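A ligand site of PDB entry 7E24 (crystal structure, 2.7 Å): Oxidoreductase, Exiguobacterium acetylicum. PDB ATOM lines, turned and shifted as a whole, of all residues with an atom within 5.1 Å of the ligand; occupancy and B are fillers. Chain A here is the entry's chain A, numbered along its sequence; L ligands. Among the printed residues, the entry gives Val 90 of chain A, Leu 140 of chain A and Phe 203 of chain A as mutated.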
ATOM      1  N   GLY A  10      13.645 -24.447 -16.428  1.00  0.00           N
ATOM      2  CA  GLY A  10      13.070 -25.684 -16.936  1.00  0.00           C
ATOM      3  C   GLY A  10      12.759 -25.578 -18.412  1.00  0.00           C
ATOM      4  O   GLY A  10      11.655 -25.932 -18.836  1.00  0.00           O
ATOM      5  N   ALA A  11      13.722 -25.072 -19.185  1.00  0.00           N
ATOM      6  CA  ALA A  11      13.533 -24.813 -20.604  1.00  0.00           C
ATOM      7  C   ALA A  11      13.994 -25.966 -21.491  1.00  0.00           C
ATOM      8  O   ALA A  11      13.855 -25.891 -22.718  1.00  0.00           O
ATOM      9  CB  ALA A  11      14.285 -23.544 -21.000  1.00  0.00           C
ATOM     10  N   SER A  12      14.541 -27.006 -20.910  1.00  0.00           N
ATOM     11  CA  SER A  12      15.072 -28.091 -21.702  1.00  0.00           C
ATOM     12  C   SER A  12      13.993 -28.996 -22.289  1.00  0.00           C
ATOM     13  O   SER A  12      14.318 -29.804 -23.168  1.00  0.00           O
ATOM     14  CB  SER A  12      15.997 -28.911 -20.815  1.00  0.00           C
ATOM     15  OG  SER A  12      16.066 -30.243 -21.220  1.00  0.00           O
ATOM     16  N   SER A  13      12.738 -28.867 -21.848  1.00  0.00           N
ATOM     17  CA  SER A  13      11.735 -29.869 -22.174  1.00  0.00           C
ATOM     18  C   SER A  13      10.347 -29.369 -21.756  1.00  0.00           C
ATOM     19  O   SER A  13      10.170 -28.487 -20.895  1.00  0.00           O
ATOM     20  CB  SER A  13      12.108 -31.205 -21.504  1.00  0.00           C
ATOM     21  OG  SER A  13      10.971 -32.026 -21.257  1.00  0.00           O
ATOM     22  N   GLY A  14       9.347 -29.941 -22.410  1.00  0.00           N
ATOM     23  CA  GLY A  14       7.974 -29.730 -21.947  1.00  0.00           C
ATOM     24  C   GLY A  14       7.529 -28.306 -22.124  1.00  0.00           C
ATOM     25  O   GLY A  14       7.786 -27.676 -23.155  1.00  0.00           O
ATOM     26  N   ILE A  15       6.859 -27.782 -21.096  1.00  0.00           N
ATOM     27  CA  ILE A  15       6.203 -26.478 -21.200  1.00  0.00           C
ATOM     28  C   ILE A  15       7.221 -25.381 -21.431  1.00  0.00           C
ATOM     29  O   ILE A  15       7.061 -24.545 -22.319  1.00  0.00           O
ATOM     30  CB  ILE A  15       5.351 -26.208 -19.948  1.00  0.00           C
ATOM     31  CG1 ILE A  15       4.225 -27.234 -19.825  1.00  0.00           C
ATOM     32  CG2 ILE A  15       4.790 -24.810 -19.982  1.00  0.00           C
ATOM     33  CD1 ILE A  15       3.535 -27.223 -18.487  1.00  0.00           C
ATOM     34  N   GLY A  16       8.291 -25.353 -20.627  1.00  0.00           N
ATOM     35  CA  GLY A  16       9.308 -24.336 -20.811  1.00  0.00           C
ATOM     36  C   GLY A  16       9.898 -24.347 -22.201  1.00  0.00           C
ATOM     37  O   GLY A  16      10.111 -23.302 -22.814  1.00  0.00           O
ATOM     38  N   VAL A  33      17.131 -21.776 -18.760  1.00  0.00           N
ATOM     39  CA  VAL A  33      17.810 -22.397 -17.628  1.00  0.00           C
ATOM     40  C   VAL A  33      17.358 -23.834 -17.487  1.00  0.00           C
ATOM     41  O   VAL A  33      16.157 -24.117 -17.463  1.00  0.00           O
ATOM     42  CB  VAL A  33      17.555 -21.623 -16.332  1.00  0.00           C
ATOM     43  CG1 VAL A  33      18.460 -22.109 -15.243  1.00  0.00           C
ATOM     44  CG2 VAL A  33      17.779 -20.128 -16.578  1.00  0.00           C
ATOM     45  N   ALA A  34      18.311 -24.740 -17.415  1.00  0.00           N
ATOM     46  CA  ALA A  34      18.006 -26.116 -17.049  1.00  0.00           C
ATOM     47  C   ALA A  34      19.338 -26.807 -16.822  1.00  0.00           C
ATOM     48  O   ALA A  34      20.394 -26.165 -16.786  1.00  0.00           O
ATOM     49  CB  ALA A  34      17.171 -26.824 -18.121  1.00  0.00           C
ATOM     50  N   ARG A  35      19.285 -28.120 -16.643  1.00  0.00           N
ATOM     51  CA  ARG A  35      20.507 -28.842 -16.343  1.00  0.00           C
ATOM     52  C   ARG A  35      21.103 -29.467 -17.585  1.00  0.00           C
ATOM     53  O   ARG A  35      22.335 -29.542 -17.700  1.00  0.00           O
ATOM     54  CB  ARG A  35      20.284 -29.938 -15.295  1.00  0.00           C
ATOM     55  CG  ARG A  35      20.187 -29.457 -13.888  1.00  0.00           C
ATOM     56  CD  ARG A  35      19.563 -30.499 -13.014  1.00  0.00           C
ATOM     57  NE  ARG A  35      18.412 -31.131 -13.649  1.00  0.00           N
ATOM     58  CZ  ARG A  35      17.862 -32.272 -13.219  1.00  0.00           C
ATOM     59  NH1 ARG A  35      18.369 -32.890 -12.162  1.00  0.00           N
ATOM     60  NH2 ARG A  35      16.823 -32.784 -13.852  1.00  0.00           N
ATOM     61  N   ARG A  36      20.263 -29.928 -18.499  1.00  0.00           N
ATOM     62  CA  ARG A  36      20.723 -30.595 -19.707  1.00  0.00           C
ATOM     63  C   ARG A  36      21.171 -29.539 -20.690  1.00  0.00           C
ATOM     64  O   ARG A  36      20.368 -28.933 -21.407  1.00  0.00           O
ATOM     65  CB  ARG A  36      19.629 -31.481 -20.299  1.00  0.00           C
ATOM     66  CG  ARG A  36      19.462 -32.816 -19.620  1.00  0.00           C
ATOM     67  CD  ARG A  36      18.202 -33.508 -20.059  1.00  0.00           C
ATOM     68  NE  ARG A  36      17.032 -32.667 -19.830  1.00  0.00           N
ATOM     69  CZ  ARG A  36      15.777 -33.108 -19.919  1.00  0.00           C
ATOM     70  NH1 ARG A  36      15.543 -34.382 -20.216  1.00  0.00           N
ATOM     71  NH2 ARG A  36      14.761 -32.295 -19.704  1.00  0.00           N
ATOM     72  N   VAL A  61      22.290 -25.161 -14.950  1.00  0.00           N
ATOM     73  CA  VAL A  61      22.199 -24.857 -13.520  1.00  0.00           C
ATOM     74  C   VAL A  61      21.244 -25.857 -12.870  1.00  0.00           C
ATOM     75  O   VAL A  61      20.098 -26.020 -13.322  1.00  0.00           O
ATOM     76  CB  VAL A  61      21.668 -23.439 -13.266  1.00  0.00           C
ATOM     77  CG1 VAL A  61      21.520 -23.202 -11.789  1.00  0.00           C
ATOM     78  CG2 VAL A  61      22.579 -22.406 -13.864  1.00  0.00           C
ATOM     79  N   ASP A  62      21.698 -26.547 -11.822  1.00  0.00           N
ATOM     80  CA  ASP A  62      20.816 -27.328 -10.959  1.00  0.00           C
ATOM     81  C   ASP A  62      20.224 -26.367  -9.948  1.00  0.00           C
ATOM     82  O   ASP A  62      20.944 -25.837  -9.093  1.00  0.00           O
ATOM     83  CB  ASP A  62      21.606 -28.447 -10.253  1.00  0.00           C
ATOM     84  CG  ASP A  62      20.720 -29.395  -9.431  1.00  0.00           C
ATOM     85  OD1 ASP A  62      19.582 -29.032  -9.073  1.00  0.00           O
ATOM     86  OD2 ASP A  62      21.175 -30.532  -9.148  1.00  0.00           O
ATOM     87  N   LEU A  63      18.919 -26.094 -10.068  1.00  0.00           N
ATOM     88  CA  LEU A  63      18.247 -25.116  -9.206  1.00  0.00           C
ATOM     89  C   LEU A  63      17.777 -25.713  -7.884  1.00  0.00           C
ATOM     90  O   LEU A  63      17.199 -24.993  -7.058  1.00  0.00           O
ATOM     91  CB  LEU A  63      17.064 -24.480  -9.957  1.00  0.00           C
ATOM     92  CG  LEU A  63      17.401 -23.746 -11.251  1.00  0.00           C
ATOM     93  CD1 LEU A  63      16.163 -23.490 -12.112  1.00  0.00           C
ATOM     94  CD2 LEU A  63      18.072 -22.451 -10.891  1.00  0.00           C
ATOM     95  N   ALA A  64      17.988 -27.009  -7.662  1.00  0.00           N
ATOM     96  CA  ALA A  64      17.682 -27.629  -6.381  1.00  0.00           C
ATOM     97  C   ALA A  64      18.702 -27.291  -5.299  1.00  0.00           C
ATOM     98  O   ALA A  64      18.613 -27.831  -4.190  1.00  0.00           O
ATOM     99  CB  ALA A  64      17.591 -29.142  -6.562  1.00  0.00           C
ATOM    100  N   ASN A  87       9.204 -22.077 -14.138  1.00  0.00           N
ATOM    101  CA  ASN A  87       8.592 -23.278 -14.721  1.00  0.00           C
ATOM    102  C   ASN A  87       9.248 -24.578 -14.260  1.00  0.00           C
ATOM    103  O   ASN A  87       8.577 -25.611 -14.255  1.00  0.00           O
ATOM    104  CB  ASN A  87       8.630 -23.179 -16.254  1.00  0.00           C
ATOM    105  CG  ASN A  87       8.284 -24.491 -16.964  1.00  0.00           C
ATOM    106  OD1 ASN A  87       7.127 -24.875 -17.044  1.00  0.00           O
ATOM    107  ND2 ASN A  87       9.292 -25.177 -17.470  1.00  0.00           N
ATOM    108  N   ALA A  88      10.525 -24.578 -13.867  1.00  0.00           N
ATOM    109  CA  ALA A  88      11.178 -25.842 -13.538  1.00  0.00           C
ATOM    110  C   ALA A  88      10.559 -26.452 -12.285  1.00  0.00           C
ATOM    111  O   ALA A  88      10.237 -25.740 -11.333  1.00  0.00           O
ATOM    112  CB  ALA A  88      12.676 -25.661 -13.353  1.00  0.00           C
ATOM    113  N   GLY A  89      10.350 -27.755 -12.322  1.00  0.00           N
ATOM    114  CA  GLY A  89       9.668 -28.437 -11.250  1.00  0.00           C
ATOM    115  C   GLY A  89       9.594 -29.907 -11.575  1.00  0.00           C
ATOM    116  O   GLY A  89       9.740 -30.314 -12.730  1.00  0.00           O
ATOM    117  N   VAL A  90       9.385 -30.719 -10.521  1.00  0.00           N
ATOM    118  CA  VAL A  90       9.329 -32.172 -10.687  1.00  0.00           C
ATOM    119  C   VAL A  90       8.155 -32.712  -9.880  1.00  0.00           C
ATOM    120  O   VAL A  90       7.575 -32.023  -9.044  1.00  0.00           O
ATOM    121  CB  VAL A  90      10.646 -32.851 -10.266  1.00  0.00           C
ATOM    122  CG1 VAL A  90      11.827 -32.237 -10.999  1.00  0.00           C
ATOM    123  CG2 VAL A  90      10.825 -32.781  -8.779  1.00  0.00           C
ATOM    124  N   LYS A 106      14.735 -32.933  -2.524  1.00  0.00           N
ATOM    125  CA  LYS A 106      15.153 -32.208  -3.725  1.00  0.00           C
ATOM    126  C   LYS A 106      13.960 -31.555  -4.388  1.00  0.00           C
ATOM    127  O   LYS A 106      14.026 -30.397  -4.806  1.00  0.00           O
ATOM    128  CB  LYS A 106      15.872 -33.157  -4.660  1.00  0.00           C
ATOM    129  CG  LYS A 106      16.803 -32.524  -5.668  1.00  0.00           C
ATOM    130  CD  LYS A 106      17.132 -33.528  -6.768  1.00  0.00           C
ATOM    131  CE  LYS A 106      18.297 -33.057  -7.640  1.00  0.00           C
ATOM    132  NZ  LYS A 106      18.578 -33.950  -8.800  1.00  0.00           N
ATOM    133  N   LEU A 110      13.570 -27.513  -5.317  1.00  0.00           N
ATOM    134  CA  LEU A 110      13.265 -27.008  -6.647  1.00  0.00           C
ATOM    135  C   LEU A 110      11.878 -26.372  -6.718  1.00  0.00           C
ATOM    136  O   LEU A 110      11.747 -25.188  -7.066  1.00  0.00           O
ATOM    137  CB  LEU A 110      13.376 -28.143  -7.654  1.00  0.00           C
ATOM    138  CG  LEU A 110      13.031 -27.771  -9.085  1.00  0.00           C
ATOM    139  CD1 LEU A 110      14.035 -26.751  -9.597  1.00  0.00           C
ATOM    140  CD2 LEU A 110      12.998 -29.012  -9.973  1.00  0.00           C
ATOM    141  N   ILE A 137       4.657 -21.406 -12.313  1.00  0.00           N
ATOM    142  CA  ILE A 137       3.909 -22.544 -12.828  1.00  0.00           C
ATOM    143  C   ILE A 137       3.505 -23.423 -11.659  1.00  0.00           C
ATOM    144  O   ILE A 137       4.352 -24.062 -11.009  1.00  0.00           O
ATOM    145  CB  ILE A 137       4.703 -23.327 -13.870  1.00  0.00           C
ATOM    146  CG1 ILE A 137       5.219 -22.348 -14.918  1.00  0.00           C
ATOM    147  CG2 ILE A 137       3.802 -24.414 -14.489  1.00  0.00           C
ATOM    148  CD1 ILE A 137       4.157 -21.500 -15.541  1.00  0.00           C
ATOM    149  N   SER A 138       2.205 -23.473 -11.389  1.00  0.00           N
ATOM    150  CA  SER A 138       1.614 -24.322 -10.371  1.00  0.00           C
ATOM    151  C   SER A 138       1.062 -25.571 -11.043  1.00  0.00           C
ATOM    152  O   SER A 138       1.782 -26.173 -11.845  1.00  0.00           O
ATOM    153  CB  SER A 138       0.592 -23.496  -9.564  1.00  0.00           C
ATOM    154  OG  SER A 138      -0.006 -24.245  -8.533  1.00  0.00           O
ATOM    155  N   SER A 139      -0.167 -25.994 -10.766  1.00  0.00           N
ATOM    156  CA  SER A 139      -0.804 -27.132 -11.392  1.00  0.00           C
ATOM    157  C   SER A 139      -2.244 -27.096 -10.915  1.00  0.00           C
ATOM    158  O   SER A 139      -2.558 -26.424  -9.918  1.00  0.00           O
ATOM    159  CB  SER A 139      -0.116 -28.421 -11.007  1.00  0.00           C
ATOM    160  OG  SER A 139      -0.738 -29.552 -11.582  1.00  0.00           O
ATOM    161  N   LEU A 140      -3.118 -27.812 -11.618  1.00  0.00           N
ATOM    162  CA  LEU A 140      -4.434 -28.092 -11.048  1.00  0.00           C
ATOM    163  C   LEU A 140      -4.271 -28.800  -9.718  1.00  0.00           C
ATOM    164  O   LEU A 140      -5.071 -28.612  -8.788  1.00  0.00           O
ATOM    165  CB  LEU A 140      -5.254 -28.909 -12.032  1.00  0.00           C
ATOM    166  CG  LEU A 140      -6.729 -29.124 -11.722  1.00  0.00           C
ATOM    167  CD1 LEU A 140      -7.549 -27.807 -11.558  1.00  0.00           C
ATOM    168  CD2 LEU A 140      -7.325 -30.024 -12.789  1.00  0.00           C
ATOM    169  N   TYR A 152       3.817 -33.639  -3.717  1.00  0.00           N
ATOM    170  CA  TYR A 152       3.963 -32.732  -4.860  1.00  0.00           C
ATOM    171  C   TYR A 152       2.816 -31.727  -4.918  1.00  0.00           C
ATOM    172  O   TYR A 152       3.022 -30.537  -5.194  1.00  0.00           O
ATOM    173  CB  TYR A 152       4.029 -33.537  -6.157  1.00  0.00           C
ATOM    174  CG  TYR A 152       3.698 -32.761  -7.405  1.00  0.00           C
ATOM    175  CD1 TYR A 152       4.665 -31.994  -8.054  1.00  0.00           C
ATOM    176  CD2 TYR A 152       2.435 -32.784  -7.943  1.00  0.00           C
ATOM    177  CE1 TYR A 152       4.363 -31.309  -9.199  1.00  0.00           C
ATOM    178  CE2 TYR A 152       2.129 -32.088  -9.072  1.00  0.00           C
ATOM    179  CZ  TYR A 152       3.104 -31.350  -9.710  1.00  0.00           C
ATOM    180  OH  TYR A 152       2.787 -30.647 -10.860  1.00  0.00           O
ATOM    181  N   LYS A 156       2.671 -27.443  -4.937  1.00  0.00           N
ATOM    182  CA  LYS A 156       1.913 -26.580  -5.851  1.00  0.00           C
ATOM    183  C   LYS A 156       0.873 -25.753  -5.101  1.00  0.00           C
ATOM    184  O   LYS A 156       0.505 -24.667  -5.566  1.00  0.00           O
ATOM    185  CB  LYS A 156       1.221 -27.395  -6.931  1.00  0.00           C
ATOM    186  CG  LYS A 156       2.177 -28.108  -7.855  1.00  0.00           C
ATOM    187  CD  LYS A 156       3.306 -27.178  -8.303  1.00  0.00           C
ATOM    188  CE  LYS A 156       4.166 -27.860  -9.353  1.00  0.00           C
ATOM    189  NZ  LYS A 156       4.965 -26.938 -10.166  1.00  0.00           N
ATOM    190  N   PRO A 184      -1.714 -25.718 -15.121  1.00  0.00           N
ATOM    191  CA  PRO A 184      -2.080 -26.705 -16.150  1.00  0.00           C
ATOM    192  C   PRO A 184      -2.775 -27.921 -15.547  1.00  0.00           C
ATOM    193  O   PRO A 184      -2.701 -28.168 -14.335  1.00  0.00           O
ATOM    194  CB  PRO A 184      -0.718 -27.111 -16.750  1.00  0.00           C
ATOM    195  CG  PRO A 184       0.250 -26.043 -16.317  1.00  0.00           C
ATOM    196  CD  PRO A 184      -0.269 -25.474 -15.037  1.00  0.00           C
ATOM    197  N   ALA A 185      -3.450 -28.690 -16.401  1.00  0.00           N
ATOM    198  CA  ALA A 185      -3.867 -30.040 -16.022  1.00  0.00           C
ATOM    199  C   ALA A 185      -2.927 -31.005 -16.718  1.00  0.00           C
ATOM    200  O   ALA A 185      -1.747 -30.688 -16.903  1.00  0.00           O
ATOM    201  CB  ALA A 185      -5.313 -30.334 -16.389  1.00  0.00           C
ATOM    202  N   ALA A 186      -3.380 -32.183 -17.110  1.00  0.00           N
ATOM    203  CA  ALA A 186      -2.459 -33.132 -17.734  1.00  0.00           C
ATOM    204  C   ALA A 186      -1.928 -32.534 -19.040  1.00  0.00           C
ATOM    205  O   ALA A 186      -2.715 -32.142 -19.910  1.00  0.00           O
ATOM    206  CB  ALA A 186      -3.131 -34.483 -17.987  1.00  0.00           C
ATOM    207  N   THR A 187      -0.610 -32.431 -19.140  1.00  0.00           N
ATOM    208  CA  THR A 187       0.054 -31.855 -20.303  1.00  0.00           C
ATOM    209  C   THR A 187       1.135 -32.813 -20.775  1.00  0.00           C
ATOM    210  O   THR A 187       1.942 -33.301 -19.980  1.00  0.00           O
ATOM    211  CB  THR A 187       0.661 -30.473 -19.962  1.00  0.00           C
ATOM    212  OG1 THR A 187      -0.322 -29.637 -19.345  1.00  0.00           O
ATOM    213  CG2 THR A 187       1.214 -29.779 -21.206  1.00  0.00           C
ATOM    214  N   THR A 189       4.270 -34.125 -21.675  1.00  0.00           N
ATOM    215  CA  THR A 189       5.679 -33.768 -21.507  1.00  0.00           C
ATOM    216  C   THR A 189       6.375 -34.952 -20.854  1.00  0.00           C
ATOM    217  O   THR A 189       5.802 -36.033 -20.696  1.00  0.00           O
ATOM    218  CB  THR A 189       5.847 -32.525 -20.623  1.00  0.00           C
ATOM    219  OG1 THR A 189       5.457 -32.851 -19.282  1.00  0.00           O
ATOM    220  CG2 THR A 189       5.032 -31.354 -21.131  1.00  0.00           C
ATOM    221  N   GLU A 190       7.619 -34.729 -20.421  1.00  0.00           N
ATOM    222  CA  GLU A 190       8.402 -35.743 -19.746  1.00  0.00           C
ATOM    223  C   GLU A 190       8.023 -35.910 -18.279  1.00  0.00           C
ATOM    224  O   GLU A 190       8.577 -36.775 -17.599  1.00  0.00           O
ATOM    225  CB  GLU A 190       9.878 -35.391 -19.827  1.00  0.00           C
ATOM    226  CG  GLU A 190      10.552 -35.767 -21.109  1.00  0.00           C
ATOM    227  CD  GLU A 190      11.880 -35.050 -21.264  1.00  0.00           C
ATOM    228  OE1 GLU A 190      12.324 -34.413 -20.281  1.00  0.00           O
ATOM    229  OE2 GLU A 190      12.478 -35.152 -22.352  1.00  0.00           O
ATOM    230  N   PHE A 191       7.078 -35.108 -17.794  1.00  0.00           N
ATOM    231  CA  PHE A 191       6.890 -34.943 -16.361  1.00  0.00           C
ATOM    232  C   PHE A 191       6.588 -36.278 -15.692  1.00  0.00           C
ATOM    233  O   PHE A 191       7.224 -36.637 -14.694  1.00  0.00           O
ATOM    234  CB  PHE A 191       5.768 -33.944 -16.099  1.00  0.00           C
ATOM    235  CG  PHE A 191       5.339 -33.848 -14.666  1.00  0.00           C
ATOM    236  CD1 PHE A 191       4.392 -34.734 -14.152  1.00  0.00           C
ATOM    237  CD2 PHE A 191       5.800 -32.826 -13.844  1.00  0.00           C
ATOM    238  CE1 PHE A 191       3.960 -34.639 -12.847  1.00  0.00           C
ATOM    239  CE2 PHE A 191       5.376 -32.724 -12.518  1.00  0.00           C
ATOM    240  CZ  PHE A 191       4.446 -33.633 -12.020  1.00  0.00           C
ATOM    241  N   ARG A 194       9.645 -38.621 -15.491  1.00  0.00           N
ATOM    242  CA  ARG A 194      10.536 -38.233 -14.391  1.00  0.00           C
ATOM    243  C   ARG A 194       9.911 -38.610 -13.048  1.00  0.00           C
ATOM    244  O   ARG A 194      10.608 -39.098 -12.141  1.00  0.00           O
ATOM    245  CB  ARG A 194      10.818 -36.734 -14.394  1.00  0.00           C
ATOM    246  CG  ARG A 194      11.165 -36.141 -15.719  1.00  0.00           C
ATOM    247  CD  ARG A 194      12.134 -37.005 -16.524  1.00  0.00           C
ATOM    248  NE  ARG A 194      13.557 -36.710 -16.292  1.00  0.00           N
ATOM    249  CZ  ARG A 194      14.188 -35.555 -16.569  1.00  0.00           C
ATOM    250  NH1 ARG A 194      13.544 -34.511 -17.088  1.00  0.00           N
ATOM    251  NH2 ARG A 194      15.484 -35.447 -16.305  1.00  0.00           N
ATOM    252  N   PHE A 203       0.733 -40.681 -23.013  1.00  0.00           N
ATOM    253  CA  PHE A 203      -0.504 -39.933 -22.783  1.00  0.00           C
ATOM    254  C   PHE A 203      -1.577 -40.361 -23.785  1.00  0.00           C
ATOM    255  O   PHE A 203      -2.736 -40.568 -23.409  1.00  0.00           O
ATOM    256  CB  PHE A 203      -0.260 -38.422 -22.920  1.00  0.00           C
ATOM    257  CG  PHE A 203       0.467 -37.792 -21.754  1.00  0.00           C
ATOM    258  CD1 PHE A 203       1.835 -38.002 -21.576  1.00  0.00           C
ATOM    259  CD2 PHE A 203      -0.200 -36.947 -20.879  1.00  0.00           C
ATOM    260  CE1 PHE A 203       2.512 -37.396 -20.520  1.00  0.00           C
ATOM    261  CE2 PHE A 203       0.485 -36.331 -19.829  1.00  0.00           C
ATOM    262  CZ  PHE A 203       1.847 -36.558 -19.639  1.00  0.00           C
HETATM  263  P1  LIG L   1       9.287 -31.739 -18.015  1.00  0.00           P
HETATM  264  O1  LIG L   1       9.129 -31.886 -19.489  1.00  0.00           O
HETATM  265  O2  LIG L   1       9.898 -32.864 -17.250  1.00  0.00           O
HETATM  266  O3  LIG L   1      10.084 -30.403 -17.704  1.00  0.00           O
HETATM  267  C1  LIG L   1      10.659 -30.111 -16.410  1.00  0.00           C
HETATM  268  C2  LIG L   1      11.794 -29.136 -16.646  1.00  0.00           C
HETATM  269  O4  LIG L   1      12.472 -28.832 -15.398  1.00  0.00           O
HETATM  270  C3  LIG L   1      12.882 -29.646 -17.599  1.00  0.00           C
HETATM  271  O5  LIG L   1      13.290 -28.580 -18.447  1.00  0.00           O
HETATM  272  C4  LIG L   1      14.032 -29.973 -16.656  1.00  0.00           C
HETATM  273  O6  LIG L   1      15.192 -29.835 -17.468  1.00  0.00           O
HETATM  274  C5  LIG L   1      13.857 -28.874 -15.612  1.00  0.00           C
HETATM  275  N1  LIG L   1      14.479 -29.203 -14.333  1.00  0.00           N
HETATM  276  C6  LIG L   1      14.196 -30.294 -13.549  1.00  0.00           C
HETATM  277  N2  LIG L   1      14.896 -30.344 -12.449  1.00  0.00           N
HETATM  278  C7  LIG L   1      15.697 -29.210 -12.497  1.00  0.00           C
HETATM  279  C8  LIG L   1      16.671 -28.701 -11.609  1.00  0.00           C
HETATM  280  N3  LIG L   1      17.008 -29.287 -10.467  1.00  0.00           N
HETATM  281  N4  LIG L   1      17.285 -27.543 -11.957  1.00  0.00           N
HETATM  282  C9  LIG L   1      16.936 -26.952 -13.106  1.00  0.00           C
HETATM  283  N5  LIG L   1      16.047 -27.346 -14.021  1.00  0.00           N
HETATM  284  C10 LIG L   1      15.450 -28.494 -13.650  1.00  0.00           C
HETATM  285  O7  LIG L   1       7.840 -31.440 -17.408  1.00  0.00           O
HETATM  286  P2  LIG L   1       6.722 -30.299 -17.549  1.00  0.00           P
HETATM  287  O8  LIG L   1       5.380 -30.943 -17.493  1.00  0.00           O
HETATM  288  O9  LIG L   1       7.035 -29.396 -18.696  1.00  0.00           O
HETATM  289  O10 LIG L   1       6.968 -29.509 -16.183  1.00  0.00           O
HETATM  290  C11 LIG L   1       7.103 -28.080 -16.197  1.00  0.00           C
HETATM  291  C12 LIG L   1       6.260 -27.511 -15.081  1.00  0.00           C
HETATM  292  O11 LIG L   1       4.895 -27.900 -15.316  1.00  0.00           O
HETATM  293  C13 LIG L   1       6.563 -28.026 -13.668  1.00  0.00           C
HETATM  294  O12 LIG L   1       6.421 -26.948 -12.754  1.00  0.00           O
HETATM  295  C14 LIG L   1       5.443 -29.052 -13.466  1.00  0.00           C
HETATM  296  O13 LIG L   1       5.246 -29.407 -12.102  1.00  0.00           O
HETATM  297  C15 LIG L   1       4.301 -28.257 -14.082  1.00  0.00           C
HETATM  298  N6  LIG L   1       3.070 -29.047 -14.361  1.00  0.00           N
HETATM  299  C16 LIG L   1       3.112 -30.115 -15.219  1.00  0.00           C
HETATM  300  C17 LIG L   1       1.936 -30.744 -15.606  1.00  0.00           C
HETATM  301  C18 LIG L   1       1.942 -31.882 -16.587  1.00  0.00           C
HETATM  302  O14 LIG L   1       0.948 -32.590 -16.672  1.00  0.00           O
HETATM  303  N7  LIG L   1       3.012 -32.065 -17.345  1.00  0.00           N
HETATM  304  C19 LIG L   1       0.726 -30.311 -15.063  1.00  0.00           C
HETATM  305  C20 LIG L   1       0.716 -29.293 -14.146  1.00  0.00           C
HETATM  306  C21 LIG L   1       1.895 -28.663 -13.823  1.00  0.00           C
HETATM  307  P3  LIG L   1      16.545 -30.451 -16.867  1.00  0.00           P
HETATM  308  O15 LIG L   1      17.037 -29.475 -15.822  1.00  0.00           O
HETATM  309  O16 LIG L   1      16.180 -31.810 -16.274  1.00  0.00           O
HETATM  310  O17 LIG L   1      17.497 -30.577 -18.035  1.00  0.00           O
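The backbone NH (N) of Ser 13 is in hydrogen-bond range of an oxygen (O5) of the ligand (3.5 Å).
The guanidinium group (NH2) of Arg 35 is in salt-bridge range of an oxygen (O16) of the ligand (2.7 Å).
The guanidinium group (NH2) of Arg 194 is in salt-bridge range of an oxygen (O16) of the ligand, 3.7 Å away.
An oxygen (O8) of the ligand is in hydrogen-bond range of the side-chain hydroxyl of Thr 189 (2.6 Å).
An oxygen (O5) of the ligand lies close to the backbone carbonyl oxygen (O) of Gly 10.
N of Ser 12 is in hydrogen-bond range of O5 of the ligand (3.2 Å).
NE of Arg 36 lies within salt-bridge range of O17 of the ligand (2.8 Å).
The backbone NH (N) of Ile 15 is in hydrogen-bond range of an oxygen (O9) of the ligand, 2.9 Å away.
The side-chain hydroxyl (OH) of Tyr 152 lies within hydrogen-bond range of an oxygen (O13) of the ligand (3.0 Å).
The backbone NH of Arg 36 is in hydrogen-bond range of an oxygen (O17) of the ligand (2.9 Å).
O1 of the ligand lies within hydrogen-bond range of N of Glu 190 (3.4 Å).
N of Arg 35 sits at hydrogen-bond distance from O15 of the ligand, 2.8 Å away.
O of Thr 187 lies within hydrogen-bond range of N7 of the ligand (3.1 Å).
The side-chain amino group of Lys 156 lies within hydrogen-bond range of an oxygen (O12) of the ligand (3.0 Å).
A nitrogen (N4) of the ligand is in hydrogen-bond range of the backbone NH of Leu 63 (2.9 Å).
A nitrogen (N3) of the ligand lies within hydrogen-bond range of the side-chain carboxylate (OD1) of Asp 62, at 2.9 Å.
The side-chain hydroxyl (OG) of Ser 13 sits at hydrogen-bond distance from an oxygen (O1) of the ligand, at 2.6 Å.
An oxygen (O14) of the ligand is in hydrogen-bond range of the backbone NH (N) of Thr 187, 2.9 Å away.
O of Asn 87 is in hydrogen-bond range of O12 of the ligand (2.9 Å).
The side-chain hydroxyl (OG) of Ser 13 lies within hydrogen-bond range of the side-chain carboxylate (OE1) of Glu 190, at 2.9 Å.
N of Phe 191 sits close to OG1 of Thr 189, 3.2 Å away.
The side-chain hydroxyl of Thr 187 sits at hydrogen-bond distance from the backbone carbonyl oxygen of Ala 185.
The side-chain carboxylate of Glu 190 lies within salt-bridge range of the guanidinium group of Arg 36 (3.2 Å).
O of Gly 10 sits at hydrogen-bond distance from ND2 of Asn 87.
The side-chain hydroxyl (OG) of Ser 12 lies within hydrogen-bond range of the guanidinium group (NH2) of Arg 36, 2.9 Å away.
The backbone NH of Gly 10 lies within hydrogen-bond range of the backbone carbonyl oxygen of Val 33.
ND2 of Asn 87 lies close to N of Gly 16 (3.3 Å).
O of Val 61 sits close to N4 of the ligand (3.5 Å).
An oxygen (O14) of the ligand sits close to the backbone carbonyl oxygen (O) of Ala 185 (3.3 Å).
Merely in contact with the ligand: Ser 139 (3.0 Å), Ser 138 (3.2 Å), Phe 191 (3.3 Å), Leu 110 (3.4 Å), Gly 14 (3.4 Å), Ala 34 (3.5 Å), Pro 184 (3.6 Å), Ala 186 (3.6 Å), Ala 11 (3.6 Å), Ala 64 (3.7 Å), Ile 137 (3.7 Å), Ala 88 (3.8 Å), Gly 89 (3.8 Å) and Val 90 (3.9 Å).
The nearest printed residue that does not touch the ligand is Gly 16 (4.7 Å).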
